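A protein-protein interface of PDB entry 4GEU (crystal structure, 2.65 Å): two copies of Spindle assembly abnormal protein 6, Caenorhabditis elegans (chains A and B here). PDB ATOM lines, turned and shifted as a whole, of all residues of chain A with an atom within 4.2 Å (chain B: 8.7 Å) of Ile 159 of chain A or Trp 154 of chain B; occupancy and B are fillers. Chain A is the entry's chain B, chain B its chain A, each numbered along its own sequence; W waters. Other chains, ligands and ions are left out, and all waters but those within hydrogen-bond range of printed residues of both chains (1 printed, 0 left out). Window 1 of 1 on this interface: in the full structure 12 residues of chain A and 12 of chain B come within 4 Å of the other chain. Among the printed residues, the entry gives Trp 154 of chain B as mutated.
Water W1 bridges the side-chain hydroxyl (OG1) of Thr 84 of chain A and the backbone carbonyl oxygen (O) of Ser 155 of chain B.
The backbone NH (N) of Ser 155 of chain B is in hydrogen-bond range of the side-chain hydroxyl (OG1) of Thr 84 of chain A (3.3 Å). O of Trp 154 of chain B lies within hydrogen-bond range of N of Thr 84 of chain A (2.7 Å).
Positions printed for both chains: 150 and 157. Of the 10 pairs that touch across the chains among the printed residues, none has its exchanged pair printed and touching as well.
The side-chain hydroxyl of Ser 155 of chain B lies close to the backbone NH of Gly 157 of chain B (3.4 Å). The backbone carbonyl oxygen of Leu 148 of chain A is in hydrogen-bond range of the backbone NH of Ile 159 of chain A, at 2.7 Å. The backbone carbonyl oxygen of Lys 156 of chain B sits close to the backbone NH of Lys 151 of chain B (3.4 Å). The side-chain hydroxyl (OG1) of Thr 152 of chain B sits close to the backbone NH (N) of Trp 154 of chain B (3.1 Å). The side-chain hydroxyl (OG1) of Thr 152 of chain B lies within hydrogen-bond range of the side-chain hydroxyl (OG) of Ser 155 of chain B (2.7 Å).
Of the printed residues of chain B, Ile 159 of chain A touches Trp 154 (3.4 Å). Of chain A, only Leu 83 (3.2 Å), Thr 84 (2.7 Å), Val 85 (3.7 Å), Val 93 (3.9 Å), Leu 98 (3.7 Å) and Ile 159 (3.4 Å) come within 4 Å of Trp 154 of chain B. Printed residues of chain A within 4 Å of Ser 155 of chain B: Asp 82 (3.3 Å) and Thr 84 (3.3 Å). Printed residues of chain B within 4 Å of Thr 84 of chain A: Trp 154, Ser 155 and Lys 156. Printed residues of chain B within 4 Å of Val 85 of chain A: Trp 154. Of the printed residues of chain B, Asp 82 of chain A touches Ser 155. Gly 157 of chain B touches none of the printed residues of chain A. Thr 152 of chain B touches none of the printed residues of chain A. The nearest residue of chain B that does not touch Ile 159 of chain A is Thr 152 of chain B (6.5 Å).
Among the printed residues, pairs that only touch across the chains: Asp 82 of chain A with Ser 155 of chain B (3.3 Å), Leu 83 of chain A with Trp 154 of chain B (3.2 Å), Thr 84 of chain A with Lys 156 of chain B (3.7 Å), Val 85 of chain A with Trp 154 of chain B (3.7 Å), Val 93 of chain A with Pro 153 of chain B (3.7 Å), Val 93 of chain A with Trp 154 of chain B (3.9 Å), Leu 98 of chain A with Trp 154 of chain B (3.7 Å) and Ile 159 of chain A with Trp 154 of chain B (3.4 Å).
Hydrophobic or aromatic side chains of chain A that line the printed part of chain B: Leu 83, Val 93, Leu 98 and Ile 159. Along chain B the printed residues that touch a printed residue of chain A span positions 153 to 156. Among the printed residues, 10 pairs touch across the chains. Among the printed residues, no Asp or Glu carboxylate lies within 4 Å of a Lys or Arg side-chain nitrogen of the other chain.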
ATOM      1  N   HIS A  81      26.748  -6.303  16.387  1.00  0.00           N
ATOM      2  CA  HIS A  81      26.594  -7.168  15.213  1.00  0.00           C
ATOM      3  C   HIS A  81      26.296  -6.440  13.928  1.00  0.00           C
ATOM      4  O   HIS A  81      25.859  -7.078  12.956  1.00  0.00           O
ATOM      5  CB  HIS A  81      25.485  -8.178  15.465  1.00  0.00           C
ATOM      6  CG  HIS A  81      25.783  -9.087  16.606  1.00  0.00           C
ATOM      7  ND1 HIS A  81      25.276  -8.842  17.871  1.00  0.00           N
ATOM      8  CD2 HIS A  81      26.580 -10.179  16.653  1.00  0.00           C
ATOM      9  CE1 HIS A  81      25.763  -9.805  18.640  1.00  0.00           C
ATOM     10  NE2 HIS A  81      26.560 -10.625  17.953  1.00  0.00           N
ATOM     11  N   ASP A  82      26.525  -5.115  13.919  1.00  0.00           N
ATOM     12  CA  ASP A  82      26.343  -4.230  12.773  1.00  0.00           C
ATOM     13  C   ASP A  82      24.965  -4.394  12.145  1.00  0.00           C
ATOM     14  O   ASP A  82      24.831  -4.449  10.923  1.00  0.00           O
ATOM     15  CB  ASP A  82      27.471  -4.433  11.753  1.00  0.00           C
ATOM     16  CG  ASP A  82      28.806  -4.033  12.341  1.00  0.00           C
ATOM     17  OD1 ASP A  82      28.940  -2.863  12.738  1.00  0.00           O
ATOM     18  OD2 ASP A  82      29.655  -4.933  12.561  1.00  0.00           O
ATOM     19  N   LEU A  83      23.940  -4.441  12.989  1.00  0.00           N
ATOM     20  CA  LEU A  83      22.564  -4.524  12.523  1.00  0.00           C
ATOM     21  C   LEU A  83      22.131  -3.137  12.057  1.00  0.00           C
ATOM     22  O   LEU A  83      22.459  -2.145  12.713  1.00  0.00           O
ATOM     23  CB  LEU A  83      21.621  -5.059  13.637  1.00  0.00           C
ATOM     24  CG  LEU A  83      21.910  -6.459  14.171  1.00  0.00           C
ATOM     25  CD1 LEU A  83      20.999  -6.793  15.366  1.00  0.00           C
ATOM     26  CD2 LEU A  83      21.631  -7.458  13.130  1.00  0.00           C
ATOM     27  N   THR A  84      21.401  -3.052  10.949  1.00  0.00           N
ATOM     28  CA  THR A  84      20.896  -1.756  10.464  1.00  0.00           C
ATOM     29  C   THR A  84      19.442  -1.582  10.840  1.00  0.00           C
ATOM     30  O   THR A  84      19.008  -0.478  11.122  1.00  0.00           O
ATOM     31  CB  THR A  84      21.069  -1.607   8.957  1.00  0.00           C
ATOM     32  OG1 THR A  84      20.451  -2.721   8.286  1.00  0.00           O
ATOM     33  CG2 THR A  84      22.532  -1.407   8.542  1.00  0.00           C
ATOM     34  N   VAL A  85      18.703  -2.673  10.897  1.00  0.00           N
ATOM     35  CA  VAL A  85      17.272  -2.725  11.228  1.00  0.00           C
ATOM     36  C   VAL A  85      16.989  -2.140  12.639  1.00  0.00           C
ATOM     37  O   VAL A  85      17.774  -2.358  13.568  1.00  0.00           O
ATOM     38  CB  VAL A  85      16.801  -4.191  11.061  1.00  0.00           C
ATOM     39  CG1 VAL A  85      17.505  -5.170  12.010  1.00  0.00           C
ATOM     40  CG2 VAL A  85      15.310  -4.319  11.105  1.00  0.00           C
ATOM     41  N   VAL A  93      12.054  -9.050  10.573  1.00  0.00           N
ATOM     42  CA  VAL A  93      13.123  -9.376   9.606  1.00  0.00           C
ATOM     43  C   VAL A  93      13.676 -10.812   9.847  1.00  0.00           C
ATOM     44  O   VAL A  93      13.728 -11.628   8.911  1.00  0.00           O
ATOM     45  CB  VAL A  93      14.224  -8.264   9.644  1.00  0.00           C
ATOM     46  CG1 VAL A  93      15.524  -8.706   9.013  1.00  0.00           C
ATOM     47  CG2 VAL A  93      13.731  -7.003   8.963  1.00  0.00           C
ATOM     48  N   LEU A  98      14.673 -15.554   8.115  1.00  0.00           N
ATOM     49  CA  LEU A  98      15.617 -16.551   8.564  1.00  0.00           C
ATOM     50  C   LEU A  98      14.985 -17.692   9.318  1.00  0.00           C
ATOM     51  O   LEU A  98      15.400 -18.839   9.147  1.00  0.00           O
ATOM     52  CB  LEU A  98      16.708 -15.897   9.419  1.00  0.00           C
ATOM     53  CG  LEU A  98      17.550 -14.856   8.719  1.00  0.00           C
ATOM     54  CD1 LEU A  98      18.224 -13.933   9.704  1.00  0.00           C
ATOM     55  CD2 LEU A  98      18.498 -15.481   7.746  1.00  0.00           C
ATOM     56  N   LEU A 148      22.453 -16.950  15.425  1.00  0.00           N
ATOM     57  CA  LEU A 148      21.778 -17.184  14.155  1.00  0.00           C
ATOM     58  C   LEU A 148      22.706 -16.853  12.991  1.00  0.00           C
ATOM     59  O   LEU A 148      23.357 -15.815  13.015  1.00  0.00           O
ATOM     60  CB  LEU A 148      20.524 -16.313  14.123  1.00  0.00           C
ATOM     61  CG  LEU A 148      19.474 -16.604  13.083  1.00  0.00           C
ATOM     62  CD1 LEU A 148      19.040 -18.049  13.115  1.00  0.00           C
ATOM     63  CD2 LEU A 148      18.304 -15.623  13.239  1.00  0.00           C
ATOM     64  N   PHE A 149      22.762 -17.730  11.980  1.00  0.00           N
ATOM     65  CA  PHE A 149      23.653 -17.634  10.832  1.00  0.00           C
ATOM     66  C   PHE A 149      22.930 -17.769   9.515  1.00  0.00           C
ATOM     67  O   PHE A 149      21.993 -18.549   9.401  1.00  0.00           O
ATOM     68  CB  PHE A 149      24.695 -18.763  10.888  1.00  0.00           C
ATOM     69  CG  PHE A 149      25.702 -18.663  12.005  1.00  0.00           C
ATOM     70  CD1 PHE A 149      25.453 -19.239  13.246  1.00  0.00           C
ATOM     71  CD2 PHE A 149      26.902 -17.985  11.821  1.00  0.00           C
ATOM     72  CE1 PHE A 149      26.377 -19.122  14.286  1.00  0.00           C
ATOM     73  CE2 PHE A 149      27.833 -17.884  12.858  1.00  0.00           C
ATOM     74  CZ  PHE A 149      27.562 -18.454  14.083  1.00  0.00           C
ATOM     75  N   SER A 150      23.390 -17.036   8.497  1.00  0.00           N
ATOM     76  CA  SER A 150      22.925 -17.192   7.125  1.00  0.00           C
ATOM     77  C   SER A 150      24.167 -17.229   6.247  1.00  0.00           C
ATOM     78  O   SER A 150      24.740 -16.190   5.949  1.00  0.00           O
ATOM     79  CB  SER A 150      21.946 -16.106   6.709  1.00  0.00           C
ATOM     80  OG  SER A 150      21.456 -16.388   5.407  1.00  0.00           O
ATOM     81  N   GLY A 157      28.390 -16.077   8.098  1.00  0.00           N
ATOM     82  CA  GLY A 157      27.250 -15.187   7.984  1.00  0.00           C
ATOM     83  C   GLY A 157      26.477 -15.037   9.262  1.00  0.00           C
ATOM     84  O   GLY A 157      25.239 -15.092   9.260  1.00  0.00           O
ATOM     85  N   LYS A 158      27.201 -14.816  10.362  1.00  0.00           N
ATOM     86  CA  LYS A 158      26.551 -14.570  11.643  1.00  0.00           C
ATOM     87  C   LYS A 158      25.638 -13.352  11.545  1.00  0.00           C
ATOM     88  O   LYS A 158      26.068 -12.287  11.094  1.00  0.00           O
ATOM     89  CB  LYS A 158      27.601 -14.360  12.743  1.00  0.00           C
ATOM     90  CG  LYS A 158      27.066 -14.380  14.174  1.00  0.00           C
ATOM     91  CD  LYS A 158      28.235 -14.553  15.145  1.00  0.00           C
ATOM     92  CE  LYS A 158      27.897 -14.330  16.593  1.00  0.00           C
ATOM     93  NZ  LYS A 158      28.997 -13.634  17.332  1.00  0.00           N
ATOM     94  N   ILE A 159      24.367 -13.512  11.915  1.00  0.00           N
ATOM     95  CA  ILE A 159      23.427 -12.396  11.994  1.00  0.00           C
ATOM     96  C   ILE A 159      23.618 -11.740  13.374  1.00  0.00           C
ATOM     97  O   ILE A 159      23.982 -10.568  13.458  1.00  0.00           O
ATOM     98  CB  ILE A 159      21.935 -12.769  11.786  1.00  0.00           C
ATOM     99  CG1 ILE A 159      21.602 -13.899  10.797  1.00  0.00           C
ATOM    100  CG2 ILE A 159      21.067 -11.543  11.652  1.00  0.00           C
ATOM    101  CD1 ILE A 159      22.034 -13.788   9.538  1.00  0.00           C
ATOM    102  N   PHE A 160      23.389 -12.510  14.455  1.00  0.00           N
ATOM    103  CA  PHE A 160      23.568 -12.009  15.815  1.00  0.00           C
ATOM    104  C   PHE A 160      23.681 -13.158  16.793  1.00  0.00           C
ATOM    105  O   PHE A 160      23.484 -14.301  16.420  1.00  0.00           O
ATOM    106  CB  PHE A 160      22.392 -11.066  16.223  1.00  0.00           C
ATOM    107  CG  PHE A 160      21.062 -11.790  16.285  1.00  0.00           C
ATOM    108  CD1 PHE A 160      20.569 -12.271  17.482  1.00  0.00           C
ATOM    109  CD2 PHE A 160      20.327 -12.026  15.131  1.00  0.00           C
ATOM    110  CE1 PHE A 160      19.364 -12.978  17.520  1.00  0.00           C
ATOM    111  CE2 PHE A 160      19.142 -12.747  15.165  1.00  0.00           C
ATOM    112  CZ  PHE A 160      18.660 -13.212  16.358  1.00  0.00           C
ATOM    113  N   SER B 150      27.689  -6.294   0.721  1.00  0.00           N
ATOM    114  CA  SER B 150      26.583  -7.000   0.088  1.00  0.00           C
ATOM    115  C   SER B 150      25.425  -6.918   1.080  1.00  0.00           C
ATOM    116  O   SER B 150      25.374  -7.672   2.064  1.00  0.00           O
ATOM    117  CB  SER B 150      26.969  -8.436  -0.271  1.00  0.00           C
ATOM    118  OG  SER B 150      25.959  -9.079  -1.027  1.00  0.00           O
ATOM    119  N   LYS B 151      24.524  -5.942   0.866  1.00  0.00           N
ATOM    120  CA  LYS B 151      23.402  -5.656   1.758  1.00  0.00           C
ATOM    121  C   LYS B 151      22.544  -6.861   2.049  1.00  0.00           C
ATOM    122  O   LYS B 151      22.323  -7.701   1.175  1.00  0.00           O
ATOM    123  CB  LYS B 151      22.523  -4.567   1.169  1.00  0.00           C
ATOM    124  CG  LYS B 151      21.751  -3.756   2.201  1.00  0.00           C
ATOM    125  CD  LYS B 151      20.925  -2.649   1.545  1.00  0.00           C
ATOM    126  CE  LYS B 151      20.051  -1.937   2.544  1.00  0.00           C
ATOM    127  NZ  LYS B 151      19.443  -0.697   1.980  1.00  0.00           N
ATOM    128  N   THR B 152      22.114  -6.970   3.313  1.00  0.00           N
ATOM    129  CA  THR B 152      21.184  -7.992   3.796  1.00  0.00           C
ATOM    130  C   THR B 152      19.958  -7.259   4.309  1.00  0.00           C
ATOM    131  O   THR B 152      20.040  -6.066   4.582  1.00  0.00           O
ATOM    132  CB  THR B 152      21.778  -8.859   4.911  1.00  0.00           C
ATOM    133  OG1 THR B 152      21.711  -8.120   6.117  1.00  0.00           O
ATOM    134  CG2 THR B 152      23.152  -9.326   4.653  1.00  0.00           C
ATOM    135  N   PRO B 153      18.838  -7.937   4.551  1.00  0.00           N
ATOM    136  CA  PRO B 153      17.685  -7.232   5.142  1.00  0.00           C
ATOM    137  C   PRO B 153      17.931  -6.692   6.566  1.00  0.00           C
ATOM    138  O   PRO B 153      17.091  -5.951   7.052  1.00  0.00           O
ATOM    139  CB  PRO B 153      16.591  -8.312   5.190  1.00  0.00           C
ATOM    140  CG  PRO B 153      17.048  -9.415   4.296  1.00  0.00           C
ATOM    141  CD  PRO B 153      18.532  -9.358   4.270  1.00  0.00           C
ATOM    142  N   TRP B 154      19.037  -7.045   7.234  1.00  0.00           N
ATOM    143  CA  TRP B 154      19.313  -6.664   8.626  1.00  0.00           C
ATOM    144  C   TRP B 154      20.643  -5.931   8.807  1.00  0.00           C
ATOM    145  O   TRP B 154      20.924  -5.519   9.925  1.00  0.00           O
ATOM    146  CB  TRP B 154      19.314  -7.944   9.539  1.00  0.00           C
ATOM    147  CG  TRP B 154      20.212  -9.044   9.022  1.00  0.00           C
ATOM    148  CD1 TRP B 154      21.566  -9.127   9.165  1.00  0.00           C
ATOM    149  CD2 TRP B 154      19.835 -10.121   8.149  1.00  0.00           C
ATOM    150  NE1 TRP B 154      22.058 -10.206   8.455  1.00  0.00           N
ATOM    151  CE2 TRP B 154      21.020 -10.821   7.806  1.00  0.00           C
ATOM    152  CE3 TRP B 154      18.609 -10.559   7.614  1.00  0.00           C
ATOM    153  CZ2 TRP B 154      21.025 -11.895   6.906  1.00  0.00           C
ATOM    154  CZ3 TRP B 154      18.602 -11.681   6.793  1.00  0.00           C
ATOM    155  CH2 TRP B 154      19.799 -12.320   6.428  1.00  0.00           C
ATOM    156  N   SER B 155      21.475  -5.801   7.752  1.00  0.00           N
ATOM    157  CA  SER B 155      22.806  -5.223   7.905  1.00  0.00           C
ATOM    158  C   SER B 155      23.369  -4.629   6.617  1.00  0.00           C
ATOM    159  O   SER B 155      22.822  -4.857   5.529  1.00  0.00           O
ATOM    160  CB  SER B 155      23.772  -6.309   8.370  1.00  0.00           C
ATOM    161  OG  SER B 155      23.921  -7.297   7.363  1.00  0.00           O
ATOM    162  N   LYS B 156      24.529  -3.905   6.741  1.00  0.00           N
ATOM    163  CA  LYS B 156      25.212  -3.387   5.574  1.00  0.00           C
ATOM    164  C   LYS B 156      25.839  -4.557   4.826  1.00  0.00           C
ATOM    165  O   LYS B 156      25.981  -4.485   3.620  1.00  0.00           O
ATOM    166  CB  LYS B 156      26.280  -2.332   5.917  1.00  0.00           C
ATOM    167  CG  LYS B 156      25.783  -1.056   6.591  1.00  0.00           C
ATOM    168  CD  LYS B 156      26.492   0.220   6.084  1.00  0.00           C
ATOM    169  CE  LYS B 156      27.873   0.536   6.663  1.00  0.00           C
ATOM    170  NZ  LYS B 156      28.632   1.543   5.839  1.00  0.00           N
ATOM    171  N   GLY B 157      26.218  -5.614   5.531  1.00  0.00           N
ATOM    172  CA  GLY B 157      26.793  -6.791   4.915  1.00  0.00           C
ATOM    173  C   GLY B 157      28.216  -6.573   4.436  1.00  0.00           C
ATOM    174  O   GLY B 157      28.565  -6.942   3.303  1.00  0.00           O
HETATM  175  O   HOH W   1      21.427  -1.752   5.457  1.00  0.00           O
